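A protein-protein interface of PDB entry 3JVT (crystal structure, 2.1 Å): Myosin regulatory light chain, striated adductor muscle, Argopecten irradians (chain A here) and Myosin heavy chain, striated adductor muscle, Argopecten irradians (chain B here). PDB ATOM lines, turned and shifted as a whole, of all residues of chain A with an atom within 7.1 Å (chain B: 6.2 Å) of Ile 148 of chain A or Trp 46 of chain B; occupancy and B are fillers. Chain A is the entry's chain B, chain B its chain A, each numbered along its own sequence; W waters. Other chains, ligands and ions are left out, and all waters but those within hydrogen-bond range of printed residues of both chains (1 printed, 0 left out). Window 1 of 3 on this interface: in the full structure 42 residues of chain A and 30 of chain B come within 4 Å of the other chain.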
ATOM      1  N   THR A  83     -34.399   8.259 -24.685  1.00  0.00           N
ATOM      2  CA  THR A  83     -33.010   8.480 -25.055  1.00  0.00           C
ATOM      3  C   THR A  83     -32.874   8.372 -26.544  1.00  0.00           C
ATOM      4  O   THR A  83     -33.699   7.752 -27.217  1.00  0.00           O
ATOM      5  CB  THR A  83     -32.034   7.512 -24.394  1.00  0.00           C
ATOM      6  OG1 THR A  83     -32.350   6.162 -24.757  1.00  0.00           O
ATOM      7  CG2 THR A  83     -32.075   7.720 -22.873  1.00  0.00           C
ATOM      8  N   ASP A  84     -31.818   8.983 -27.059  1.00  0.00           N
ATOM      9  CA  ASP A  84     -31.613   8.989 -28.490  1.00  0.00           C
ATOM     10  C   ASP A  84     -31.047   7.677 -28.982  1.00  0.00           C
ATOM     11  O   ASP A  84     -30.448   6.917 -28.222  1.00  0.00           O
ATOM     12  CB  ASP A  84     -30.688  10.146 -28.882  1.00  0.00           C
ATOM     13  CG  ASP A  84     -31.389  11.497 -28.845  1.00  0.00           C
ATOM     14  OD1 ASP A  84     -31.120  12.296 -27.924  1.00  0.00           O
ATOM     15  OD2 ASP A  84     -32.217  11.761 -29.742  1.00  0.00           O
ATOM     16  N   GLU A  86     -28.608   5.116 -31.159  1.00  0.00           N
ATOM     17  CA  GLU A  86     -27.201   4.981 -31.497  1.00  0.00           C
ATOM     18  C   GLU A  86     -26.885   5.812 -32.724  1.00  0.00           C
ATOM     19  O   GLU A  86     -25.876   6.506 -32.774  1.00  0.00           O
ATOM     20  CB  GLU A  86     -26.884   3.516 -31.777  1.00  0.00           C
ATOM     21  CG  GLU A  86     -25.698   2.976 -31.024  1.00  0.00           C
ATOM     22  CD  GLU A  86     -24.752   2.223 -31.925  1.00  0.00           C
ATOM     23  OE1 GLU A  86     -24.248   2.830 -32.885  1.00  0.00           O
ATOM     24  OE2 GLU A  86     -24.515   1.030 -31.684  1.00  0.00           O
ATOM     25  N   ILE A  89     -26.998   9.661 -31.951  1.00  0.00           N
ATOM     26  CA  ILE A  89     -25.887  10.069 -31.119  1.00  0.00           C
ATOM     27  C   ILE A  89     -24.632  10.096 -31.980  1.00  0.00           C
ATOM     28  O   ILE A  89     -23.858  11.051 -31.930  1.00  0.00           O
ATOM     29  CB  ILE A  89     -25.752   9.099 -29.918  1.00  0.00           C
ATOM     30  CG1 ILE A  89     -26.967   9.308 -28.986  1.00  0.00           C
ATOM     31  CG2 ILE A  89     -24.427   9.328 -29.198  1.00  0.00           C
ATOM     32  CD1 ILE A  89     -27.179   8.258 -27.899  1.00  0.00           C
ATOM     33  N   PHE A  93     -22.058  13.333 -32.883  1.00  0.00           N
ATOM     34  CA  PHE A  93     -20.597  13.369 -32.777  1.00  0.00           C
ATOM     35  C   PHE A  93     -19.953  13.695 -34.145  1.00  0.00           C
ATOM     36  O   PHE A  93     -19.030  14.496 -34.239  1.00  0.00           O
ATOM     37  CB  PHE A  93     -20.087  12.009 -32.311  1.00  0.00           C
ATOM     38  CG  PHE A  93     -20.080  11.821 -30.822  1.00  0.00           C
ATOM     39  CD1 PHE A  93     -20.796  10.791 -30.237  1.00  0.00           C
ATOM     40  CD2 PHE A  93     -19.262  12.619 -30.015  1.00  0.00           C
ATOM     41  CE1 PHE A  93     -20.692  10.534 -28.858  1.00  0.00           C
ATOM     42  CE2 PHE A  93     -19.149  12.379 -28.650  1.00  0.00           C
ATOM     43  CZ  PHE A  93     -19.858  11.335 -28.071  1.00  0.00           C
ATOM     44  N   GLU A 124     -18.634  14.615 -13.790  1.00  0.00           N
ATOM     45  CA  GLU A 124     -19.210  14.049 -15.019  1.00  0.00           C
ATOM     46  C   GLU A 124     -18.073  13.781 -16.001  1.00  0.00           C
ATOM     47  O   GLU A 124     -18.020  12.746 -16.675  1.00  0.00           O
ATOM     48  CB  GLU A 124     -20.242  15.029 -15.621  1.00  0.00           C
ATOM     49  CG  GLU A 124     -21.552  15.069 -14.818  1.00  0.00           C
ATOM     50  CD  GLU A 124     -22.524  16.166 -15.224  1.00  0.00           C
ATOM     51  OE1 GLU A 124     -22.079  17.258 -15.636  1.00  0.00           O
ATOM     52  OE2 GLU A 124     -23.746  15.946 -15.097  1.00  0.00           O
ATOM     53  N   MET A 127     -16.097  10.768 -14.714  1.00  0.00           N
ATOM     54  CA  MET A 127     -16.832   9.526 -14.953  1.00  0.00           C
ATOM     55  C   MET A 127     -16.937   9.187 -16.434  1.00  0.00           C
ATOM     56  O   MET A 127     -16.905   8.015 -16.810  1.00  0.00           O
ATOM     57  CB  MET A 127     -18.253   9.604 -14.384  1.00  0.00           C
ATOM     58  CG  MET A 127     -18.363   9.528 -12.873  1.00  0.00           C
ATOM     59  SD  MET A 127     -20.049   9.102 -12.374  1.00  0.00           S
ATOM     60  CE  MET A 127     -20.830  10.733 -12.511  1.00  0.00           C
ATOM     61  N   THR A 128     -17.072  10.205 -17.275  1.00  0.00           N
ATOM     62  CA  THR A 128     -17.201   9.967 -18.709  1.00  0.00           C
ATOM     63  C   THR A 128     -15.945   9.385 -19.348  1.00  0.00           C
ATOM     64  O   THR A 128     -16.013   8.397 -20.076  1.00  0.00           O
ATOM     65  CB  THR A 128     -17.561  11.277 -19.456  1.00  0.00           C
ATOM     66  OG1 THR A 128     -18.843  11.743 -19.016  1.00  0.00           O
ATOM     67  CG2 THR A 128     -17.582  11.049 -20.963  1.00  0.00           C
ATOM     68  N   PHE A 129     -14.798   9.988 -19.077  1.00  0.00           N
ATOM     69  CA  PHE A 129     -13.588   9.504 -19.704  1.00  0.00           C
ATOM     70  C   PHE A 129     -12.872   8.334 -19.049  1.00  0.00           C
ATOM     71  O   PHE A 129     -11.893   7.813 -19.592  1.00  0.00           O
ATOM     72  CB  PHE A 129     -12.671  10.692 -19.929  1.00  0.00           C
ATOM     73  CG  PHE A 129     -13.240  11.684 -20.920  1.00  0.00           C
ATOM     74  CD1 PHE A 129     -13.015  11.525 -22.286  1.00  0.00           C
ATOM     75  CD2 PHE A 129     -14.058  12.736 -20.490  1.00  0.00           C
ATOM     76  CE1 PHE A 129     -13.591  12.397 -23.211  1.00  0.00           C
ATOM     77  CE2 PHE A 129     -14.640  13.611 -21.406  1.00  0.00           C
ATOM     78  CZ  PHE A 129     -14.404  13.442 -22.768  1.00  0.00           C
ATOM     79  N   LYS A 130     -13.357   7.910 -17.890  1.00  0.00           N
ATOM     80  CA  LYS A 130     -12.746   6.773 -17.231  1.00  0.00           C
ATOM     81  C   LYS A 130     -13.140   5.612 -18.115  1.00  0.00           C
ATOM     82  O   LYS A 130     -12.434   4.611 -18.212  1.00  0.00           O
ATOM     83  CB  LYS A 130     -13.319   6.589 -15.823  1.00  0.00           C
ATOM     84  CG  LYS A 130     -12.984   5.237 -15.204  1.00  0.00           C
ATOM     85  CD  LYS A 130     -13.729   4.978 -13.892  1.00  0.00           C
ATOM     86  CE  LYS A 130     -13.120   5.722 -12.711  1.00  0.00           C
ATOM     87  NZ  LYS A 130     -12.965   4.823 -11.519  1.00  0.00           N
ATOM     88  N   GLU A 131     -14.277   5.771 -18.776  1.00  0.00           N
ATOM     89  CA  GLU A 131     -14.806   4.730 -19.641  1.00  0.00           C
ATOM     90  C   GLU A 131     -14.462   4.910 -21.121  1.00  0.00           C
ATOM     91  O   GLU A 131     -14.491   3.950 -21.890  1.00  0.00           O
ATOM     92  CB  GLU A 131     -16.332   4.671 -19.491  1.00  0.00           C
ATOM     93  CG  GLU A 131     -16.838   4.544 -18.049  1.00  0.00           C
ATOM     94  CD  GLU A 131     -16.391   3.261 -17.365  1.00  0.00           C
ATOM     95  OE1 GLU A 131     -16.732   3.079 -16.175  1.00  0.00           O
ATOM     96  OE2 GLU A 131     -15.702   2.438 -18.009  1.00  0.00           O
ATOM     97  N   ALA A 132     -14.127   6.132 -21.511  1.00  0.00           N
ATOM     98  CA  ALA A 132     -13.841   6.446 -22.906  1.00  0.00           C
ATOM     99  C   ALA A 132     -12.774   5.667 -23.677  1.00  0.00           C
ATOM    100  O   ALA A 132     -11.674   5.428 -23.188  1.00  0.00           O
ATOM    101  CB  ALA A 132     -13.563   7.923 -23.033  1.00  0.00           C
ATOM    102  N   LYS A 143     -17.134   3.753 -31.203  1.00  0.00           N
ATOM    103  CA  LYS A 143     -17.024   2.768 -30.137  1.00  0.00           C
ATOM    104  C   LYS A 143     -17.748   3.287 -28.887  1.00  0.00           C
ATOM    105  O   LYS A 143     -18.479   2.550 -28.236  1.00  0.00           O
ATOM    106  CB  LYS A 143     -15.551   2.520 -29.793  1.00  0.00           C
ATOM    107  CG  LYS A 143     -15.283   1.156 -29.181  1.00  0.00           C
ATOM    108  CD  LYS A 143     -13.811   0.780 -29.288  1.00  0.00           C
ATOM    109  CE  LYS A 143     -13.535  -0.566 -28.635  1.00  0.00           C
ATOM    110  NZ  LYS A 143     -12.423  -0.486 -27.650  1.00  0.00           N
ATOM    111  N   PHE A 144     -17.550   4.562 -28.569  1.00  0.00           N
ATOM    112  CA  PHE A 144     -18.120   5.148 -27.364  1.00  0.00           C
ATOM    113  C   PHE A 144     -19.641   5.140 -27.377  1.00  0.00           C
ATOM    114  O   PHE A 144     -20.288   4.851 -26.357  1.00  0.00           O
ATOM    115  CB  PHE A 144     -17.599   6.571 -27.164  1.00  0.00           C
ATOM    116  CG  PHE A 144     -18.235   7.298 -26.013  1.00  0.00           C
ATOM    117  CD1 PHE A 144     -19.319   8.141 -26.217  1.00  0.00           C
ATOM    118  CD2 PHE A 144     -17.751   7.136 -24.721  1.00  0.00           C
ATOM    119  CE1 PHE A 144     -19.908   8.809 -25.158  1.00  0.00           C
ATOM    120  CE2 PHE A 144     -18.333   7.801 -23.658  1.00  0.00           C
ATOM    121  CZ  PHE A 144     -19.415   8.640 -23.875  1.00  0.00           C
ATOM    122  N   THR A 145     -20.212   5.463 -28.531  1.00  0.00           N
ATOM    123  CA  THR A 145     -21.656   5.482 -28.687  1.00  0.00           C
ATOM    124  C   THR A 145     -22.158   4.042 -28.573  1.00  0.00           C
ATOM    125  O   THR A 145     -23.184   3.783 -27.944  1.00  0.00           O
ATOM    126  CB  THR A 145     -22.055   6.151 -30.012  1.00  0.00           C
ATOM    127  OG1 THR A 145     -21.640   7.525 -29.972  1.00  0.00           O
ATOM    128  CG2 THR A 145     -23.574   6.106 -30.208  1.00  0.00           C
ATOM    129  N   ALA A 146     -21.425   3.114 -29.171  1.00  0.00           N
ATOM    130  CA  ALA A 146     -21.751   1.701 -29.058  1.00  0.00           C
ATOM    131  C   ALA A 146     -21.816   1.292 -27.577  1.00  0.00           C
ATOM    132  O   ALA A 146     -22.722   0.567 -27.156  1.00  0.00           O
ATOM    133  CB  ALA A 146     -20.679   0.861 -29.752  1.00  0.00           C
ATOM    134  N   MET A 147     -20.832   1.738 -26.803  1.00  0.00           N
ATOM    135  CA  MET A 147     -20.743   1.388 -25.391  1.00  0.00           C
ATOM    136  C   MET A 147     -21.914   1.866 -24.557  1.00  0.00           C
ATOM    137  O   MET A 147     -22.545   1.074 -23.857  1.00  0.00           O
ATOM    138  CB  MET A 147     -19.452   1.946 -24.790  1.00  0.00           C
ATOM    139  CG  MET A 147     -19.468   2.041 -23.270  1.00  0.00           C
ATOM    140  SD  MET A 147     -17.894   2.603 -22.590  1.00  0.00           S
ATOM    141  CE  MET A 147     -16.798   2.294 -23.974  1.00  0.00           C
ATOM    142  N   ILE A 148     -22.196   3.163 -24.623  1.00  0.00           N
ATOM    143  CA  ILE A 148     -23.273   3.750 -23.837  1.00  0.00           C
ATOM    144  C   ILE A 148     -24.669   3.265 -24.221  1.00  0.00           C
ATOM    145  O   ILE A 148     -25.599   3.313 -23.411  1.00  0.00           O
ATOM    146  CB  ILE A 148     -23.238   5.288 -23.905  1.00  0.00           C
ATOM    147  CG1 ILE A 148     -23.712   5.764 -25.284  1.00  0.00           C
ATOM    148  CG2 ILE A 148     -21.829   5.788 -23.619  1.00  0.00           C
ATOM    149  CD1 ILE A 148     -24.019   7.243 -25.337  1.00  0.00           C
ATOM    150  N   LYS A 149     -24.809   2.804 -25.462  1.00  0.00           N
ATOM    151  CA  LYS A 149     -26.087   2.286 -25.940  1.00  0.00           C
ATOM    152  C   LYS A 149     -26.208   0.780 -25.683  1.00  0.00           C
ATOM    153  O   LYS A 149     -27.261   0.175 -25.889  1.00  0.00           O
ATOM    154  CB  LYS A 149     -26.279   2.617 -27.423  1.00  0.00           C
ATOM    155  CG  LYS A 149     -26.460   4.104 -27.692  1.00  0.00           C
ATOM    156  CD  LYS A 149     -27.540   4.706 -26.810  1.00  0.00           C
ATOM    157  CE  LYS A 149     -28.916   4.175 -27.174  1.00  0.00           C
ATOM    158  NZ  LYS A 149     -29.997   4.881 -26.435  1.00  0.00           N
ATOM    159  N   GLY A 150     -25.118   0.192 -25.198  1.00  0.00           N
ATOM    160  CA  GLY A 150     -25.137  -1.192 -24.766  1.00  0.00           C
ATOM    161  C   GLY A 150     -24.782  -2.192 -25.831  1.00  0.00           C
ATOM    162  O   GLY A 150     -24.626  -3.379 -25.553  1.00  0.00           O
ATOM    163  N   SER A 151     -24.659  -1.709 -27.060  1.00  0.00           N
ATOM    164  CA  SER A 151     -24.319  -2.594 -28.191  1.00  0.00           C
ATOM    165  C   SER A 151     -22.843  -2.575 -28.358  1.00  0.00           C
ATOM    166  O   SER A 151     -22.334  -2.786 -29.446  1.00  0.00           O
ATOM    167  CB  SER A 151     -24.998  -2.111 -29.476  1.00  0.00           C
ATOM    168  OG  SER A 151     -24.959  -0.696 -29.572  1.00  0.00           O
ATOM    169  N   GLY A 152     -22.153  -2.349 -27.250  1.00  0.00           N
ATOM    170  CA  GLY A 152     -20.741  -2.197 -27.347  1.00  0.00           C
ATOM    171  C   GLY A 152     -19.825  -2.736 -26.273  1.00  0.00           C
ATOM    172  O   GLY A 152     -19.838  -3.912 -25.866  1.00  0.00           O
ATOM    173  N   GLU A 153     -18.989  -1.775 -25.887  1.00  0.00           N
ATOM    174  CA  GLU A 153     -17.778  -1.858 -25.132  1.00  0.00           C
ATOM    175  C   GLU A 153     -17.664  -1.594 -23.630  1.00  0.00           C
ATOM    176  O   GLU A 153     -16.584  -1.232 -23.171  1.00  0.00           O
ATOM    177  CB  GLU A 153     -16.900  -0.942 -25.964  1.00  0.00           C
ATOM    178  CG  GLU A 153     -17.634  -0.402 -27.195  1.00  0.00           C
ATOM    179  CD  GLU A 153     -17.857  -1.463 -28.274  1.00  0.00           C
ATOM    180  OE1 GLU A 153     -18.471  -2.495 -27.952  1.00  0.00           O
ATOM    181  OE2 GLU A 153     -17.417  -1.269 -29.428  1.00  0.00           O
ATOM    182  N   GLU A 154     -18.706  -1.764 -22.824  1.00  0.00           N
ATOM    183  CA  GLU A 154     -18.617  -1.454 -21.413  1.00  0.00           C
ATOM    184  C   GLU A 154     -17.973  -2.553 -20.594  1.00  0.00           C
ATOM    185  O   GLU A 154     -17.305  -2.279 -19.586  1.00  0.00           O
ATOM    186  CB  GLU A 154     -20.025  -1.161 -20.863  1.00  0.00           C
ATOM    187  CG  GLU A 154     -20.057  -0.796 -19.387  1.00  0.00           C
ATOM    188  CD  GLU A 154     -21.057   0.304 -19.083  1.00  0.00           C
ATOM    189  OE1 GLU A 154     -21.681   0.260 -18.004  1.00  0.00           O
ATOM    190  OE2 GLU A 154     -21.212   1.217 -19.922  1.00  0.00           O
ATOM    191  N   ARG B  41     -26.659  15.262 -23.316  1.00  0.00           N
ATOM    192  CA  ARG B  41     -27.839  14.621 -22.733  1.00  0.00           C
ATOM    193  C   ARG B  41     -27.745  13.097 -22.606  1.00  0.00           C
ATOM    194  O   ARG B  41     -28.026  12.539 -21.534  1.00  0.00           O
ATOM    195  CB  ARG B  41     -29.066  14.990 -23.590  1.00  0.00           C
ATOM    196  CG  ARG B  41     -30.450  14.533 -23.113  1.00  0.00           C
ATOM    197  CD  ARG B  41     -31.470  14.605 -24.284  1.00  0.00           C
ATOM    198  NE  ARG B  41     -31.198  15.720 -25.196  1.00  0.00           N
ATOM    199  CZ  ARG B  41     -31.452  15.741 -26.516  1.00  0.00           C
ATOM    200  NH1 ARG B  41     -31.131  16.820 -27.215  1.00  0.00           N
ATOM    201  NH2 ARG B  41     -32.010  14.712 -27.150  1.00  0.00           N
ATOM    202  N   ASN B  42     -27.340  12.422 -23.677  1.00  0.00           N
ATOM    203  CA  ASN B  42     -27.287  10.966 -23.618  1.00  0.00           C
ATOM    204  C   ASN B  42     -26.154  10.412 -22.759  1.00  0.00           C
ATOM    205  O   ASN B  42     -26.284   9.325 -22.196  1.00  0.00           O
ATOM    206  CB  ASN B  42     -27.266  10.399 -25.049  1.00  0.00           C
ATOM    207  CG  ASN B  42     -28.633  10.478 -25.706  1.00  0.00           C
ATOM    208  OD1 ASN B  42     -29.466   9.596 -25.530  1.00  0.00           O
ATOM    209  ND2 ASN B  42     -28.879  11.559 -26.428  1.00  0.00           N
ATOM    210  N   ILE B  43     -25.047  11.135 -22.675  1.00  0.00           N
ATOM    211  CA  ILE B  43     -23.956  10.683 -21.831  1.00  0.00           C
ATOM    212  C   ILE B  43     -24.450  10.802 -20.388  1.00  0.00           C
ATOM    213  O   ILE B  43     -24.208   9.912 -19.581  1.00  0.00           O
ATOM    214  CB  ILE B  43     -22.688  11.567 -21.996  1.00  0.00           C
ATOM    215  CG1 ILE B  43     -22.032  11.292 -23.368  1.00  0.00           C
ATOM    216  CG2 ILE B  43     -21.693  11.268 -20.874  1.00  0.00           C
ATOM    217  CD1 ILE B  43     -20.959  12.328 -23.736  1.00  0.00           C
ATOM    218  N   ARG B  44     -25.115  11.903 -20.064  1.00  0.00           N
ATOM    219  CA  ARG B  44     -25.606  12.075 -18.706  1.00  0.00           C
ATOM    220  C   ARG B  44     -26.598  10.965 -18.375  1.00  0.00           C
ATOM    221  O   ARG B  44     -26.535  10.368 -17.298  1.00  0.00           O
ATOM    222  CB  ARG B  44     -26.234  13.462 -18.535  1.00  0.00           C
ATOM    223  CG  ARG B  44     -25.200  14.534 -18.171  1.00  0.00           C
ATOM    224  CD  ARG B  44     -25.786  15.925 -18.175  1.00  0.00           C
ATOM    225  NE  ARG B  44     -24.864  16.865 -17.555  1.00  0.00           N
ATOM    226  CZ  ARG B  44     -24.553  18.054 -18.057  1.00  0.00           C
ATOM    227  NH1 ARG B  44     -23.695  18.834 -17.413  1.00  0.00           N
ATOM    228  NH2 ARG B  44     -25.107  18.464 -19.199  1.00  0.00           N
ATOM    229  N   LYS B  45     -27.509  10.690 -19.300  1.00  0.00           N
ATOM    230  CA  LYS B  45     -28.464   9.609 -19.080  1.00  0.00           C
ATOM    231  C   LYS B  45     -27.692   8.325 -18.788  1.00  0.00           C
ATOM    232  O   LYS B  45     -28.067   7.555 -17.904  1.00  0.00           O
ATOM    233  CB  LYS B  45     -29.330   9.388 -20.324  1.00  0.00           C
ATOM    234  CG  LYS B  45     -30.459  10.390 -20.509  1.00  0.00           C
ATOM    235  CD  LYS B  45     -31.650  10.076 -19.588  1.00  0.00           C
ATOM    236  CE  LYS B  45     -32.823  11.025 -19.807  1.00  0.00           C
ATOM    237  NZ  LYS B  45     -33.890  10.784 -18.758  1.00  0.00           N
ATOM    238  N   TRP B  46     -26.621   8.088 -19.543  1.00  0.00           N
ATOM    239  CA  TRP B  46     -25.825   6.882 -19.357  1.00  0.00           C
ATOM    240  C   TRP B  46     -25.160   6.879 -17.982  1.00  0.00           C
ATOM    241  O   TRP B  46     -25.079   5.834 -17.316  1.00  0.00           O
ATOM    242  CB  TRP B  46     -24.771   6.793 -20.465  1.00  0.00           C
ATOM    243  CG  TRP B  46     -23.754   5.708 -20.310  1.00  0.00           C
ATOM    244  CD1 TRP B  46     -23.949   4.362 -20.442  1.00  0.00           C
ATOM    245  CD2 TRP B  46     -22.355   5.885 -20.067  1.00  0.00           C
ATOM    246  NE1 TRP B  46     -22.759   3.693 -20.302  1.00  0.00           N
ATOM    247  CE2 TRP B  46     -21.762   4.608 -20.064  1.00  0.00           C
ATOM    248  CE3 TRP B  46     -21.545   7.007 -19.842  1.00  0.00           C
ATOM    249  CZ2 TRP B  46     -20.394   4.416 -19.860  1.00  0.00           C
ATOM    250  CZ3 TRP B  46     -20.185   6.815 -19.636  1.00  0.00           C
ATOM    251  CH2 TRP B  46     -19.628   5.527 -19.641  1.00  0.00           C
ATOM    252  N   LEU B  47     -24.680   8.046 -17.570  1.00  0.00           N
ATOM    253  CA  LEU B  47     -24.034   8.187 -16.273  1.00  0.00           C
ATOM    254  C   LEU B  47     -25.040   7.909 -15.141  1.00  0.00           C
ATOM    255  O   LEU B  47     -24.722   7.201 -14.181  1.00  0.00           O
ATOM    256  CB  LEU B  47     -23.431   9.588 -16.127  1.00  0.00           C
ATOM    257  CG  LEU B  47     -22.210   9.880 -17.022  1.00  0.00           C
ATOM    258  CD1 LEU B  47     -21.661  11.249 -16.686  1.00  0.00           C
ATOM    259  CD2 LEU B  47     -21.131   8.838 -16.793  1.00  0.00           C
ATOM    260  N   VAL B  48     -26.243   8.468 -15.249  1.00  0.00           N
ATOM    261  CA  VAL B  48     -27.278   8.230 -14.252  1.00  0.00           C
ATOM    262  C   VAL B  48     -27.617   6.732 -14.198  1.00  0.00           C
ATOM    263  O   VAL B  48     -27.684   6.140 -13.120  1.00  0.00           O
ATOM    264  CB  VAL B  48     -28.544   9.045 -14.586  1.00  0.00           C
ATOM    265  CG1 VAL B  48     -29.683   8.690 -13.636  1.00  0.00           C
ATOM    266  CG2 VAL B  48     -28.226  10.526 -14.484  1.00  0.00           C
ATOM    267  N   LEU B  49     -27.805   6.114 -15.362  1.00  0.00           N
ATOM    268  CA  LEU B  49     -28.143   4.700 -15.427  1.00  0.00           C
ATOM    269  C   LEU B  49     -27.101   3.840 -14.717  1.00  0.00           C
ATOM    270  O   LEU B  49     -27.444   2.943 -13.937  1.00  0.00           O
ATOM    271  CB  LEU B  49     -28.284   4.250 -16.888  1.00  0.00           C
ATOM    272  CG  LEU B  49     -28.721   2.802 -17.193  1.00  0.00           C
ATOM    273  CD1 LEU B  49     -30.123   2.525 -16.634  1.00  0.00           C
ATOM    274  CD2 LEU B  49     -28.728   2.578 -18.703  1.00  0.00           C
ATOM    275  N   ARG B  50     -25.829   4.126 -14.996  1.00  0.00           N
ATOM    276  CA  ARG B  50     -24.708   3.398 -14.414  1.00  0.00           C
ATOM    277  C   ARG B  50     -24.701   3.464 -12.895  1.00  0.00           C
ATOM    278  O   ARG B  50     -24.205   2.557 -12.230  1.00  0.00           O
ATOM    279  CB  ARG B  50     -23.379   3.941 -14.945  1.00  0.00           C
ATOM    280  CG  ARG B  50     -23.157   3.694 -16.424  1.00  0.00           C
ATOM    281  CD  ARG B  50     -21.673   3.702 -16.767  1.00  0.00           C
ATOM    282  NE  ARG B  50     -20.834   3.367 -15.622  1.00  0.00           N
ATOM    283  CZ  ARG B  50     -20.248   2.187 -15.434  1.00  0.00           C
ATOM    284  NH1 ARG B  50     -19.504   1.977 -14.357  1.00  0.00           N
ATOM    285  NH2 ARG B  50     -20.396   1.220 -16.324  1.00  0.00           N
ATOM    286  N   ASN B  51     -25.253   4.536 -12.349  1.00  0.00           N
ATOM    287  CA  ASN B  51     -25.299   4.679 -10.906  1.00  0.00           C
ATOM    288  C   ASN B  51     -26.635   4.269 -10.276  1.00  0.00           C
ATOM    289  O   ASN B  51     -26.837   4.435  -9.076  1.00  0.00           O
ATOM    290  CB  ASN B  51     -24.925   6.107 -10.529  1.00  0.00           C
ATOM    291  CG  ASN B  51     -23.474   6.421 -10.867  1.00  0.00           C
ATOM    292  OD1 ASN B  51     -22.581   5.617 -10.594  1.00  0.00           O
ATOM    293  ND2 ASN B  51     -23.231   7.587 -11.457  1.00  0.00           N
HETATM  294  O   HOH W   1     -32.049  12.051 -25.158  1.00  0.00           O
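OD1 of Asp 84 of chain A lies within salt-bridge range of NH2 of Arg 41 of chain B (2.7 Å).
The side-chain carboxylate (OD1) of Asp 84 of chain A is in hydrogen-bond range of the side-chain amide nitrogen (ND2) of Asn 42 of chain B (2.8 Å).
The guanidinium group of Arg 44 of chain B is in salt-bridge range of the side-chain carboxylate of Glu 124 of chain A (2.9 Å).
The indole nitrogen (NE1) of Trp 46 of chain B lies within hydrogen-bond range of the side-chain carboxylate (OE2) of Glu 154 of chain A (2.9 Å).
The side-chain carboxylate of Glu 131 of chain A is in salt-bridge range of the guanidinium group of Arg 50 of chain B, at 3.5 Å.
The guanidinium group of Arg 50 of chain B is in salt-bridge range of the side-chain carboxylate of Glu 154 of chain A (3.7 Å).
The side-chain amide nitrogen (ND2) of Asn 51 of chain B is in hydrogen-bond range of the side-chain sulfur (SD) of Met 127 of chain A, at 3.6 Å.
The side-chain amide nitrogen of Asn 51 of chain B is in hydrogen-bond range of the backbone carbonyl oxygen of Leu 47 of chain B.
The side-chain hydroxyl of Thr 83 of chain A lies within hydrogen-bond range of the side-chain amino group of Lys 149 of chain A, at 3.2 Å.
The backbone carbonyl oxygen (O) of Asp 84 of chain A is in hydrogen-bond range of the side-chain amino group (NZ) of Lys 149 of chain A.
The side-chain hydroxyl (OG1) of Thr 128 of chain A is in hydrogen-bond range of the backbone carbonyl oxygen (O) of Glu 124 of chain A (2.7 Å).
Among the printed residues, pairs that only touch across the chains: Thr 83 of chain A with Asn 42 of chain B, Thr 83 of chain A with Lys 45 of chain B, Ile 89 of chain A with Asn 42 of chain B, Glu 124 of chain A with Leu 47 of chain B, Met 127 of chain A with Leu 47 of chain B, Thr 128 of chain A with Ile 43 of chain B, Thr 128 of chain A with Leu 47 of chain B, Glu 131 of chain A with Trp 46 of chain B, Phe 144 of chain A with Ile 43 of chain B and Ile 148 of chain A with Trp 46 of chain B.
Ile 148 of chain A touches just one residue of chain B: Trp 46.
Of chain A, only Glu 131, Ile 148 and Glu 154 come within 4 Å of Trp 46 of chain B.
Of the printed residues of chain A, Ile 43 of chain B touches Thr 128 and Phe 144.
Of the printed residues of chain B, Thr 83 of chain A touches Asn 42 and Lys 45.
Leu 49 of chain B touches none of the printed residues of chain A.
The nearest residue of chain B that does not touch Ile 148 of chain A is Asn 42 of chain B (4.4 Å).
The nearest printed residue of chain B that does not touch Glu 131 of chain A is Leu 47 of chain B (6.2 Å).
Hydrophobic or aromatic side chains of chain A within 4 Å of the printed part of chain B: Ile 89, Met 127, Phe 144 and Ile 148.
Of the 11 printed residues of chain B, 9 touch a printed residue of chain A.
Printed residues of chain B that touch a printed residue of chain A: Arg 41, Asn 42, Ile 43, Arg 44, Lys 45, Trp 46, Leu 47, Arg 50 and Asn 51.
Hydrophobic or aromatic side chains of chain B that line the printed part of chain A: Ile 43, Trp 46 and Leu 47.
Water W1 lies within hydrogen-bond range of the side-chain carboxylate of Asp 84 of chain A (2.9 Å), the guanidinium group of Arg 41 of chain B (3.3 Å) and the side-chain amide nitrogen of Asn 42 of chain B (3.5 Å).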
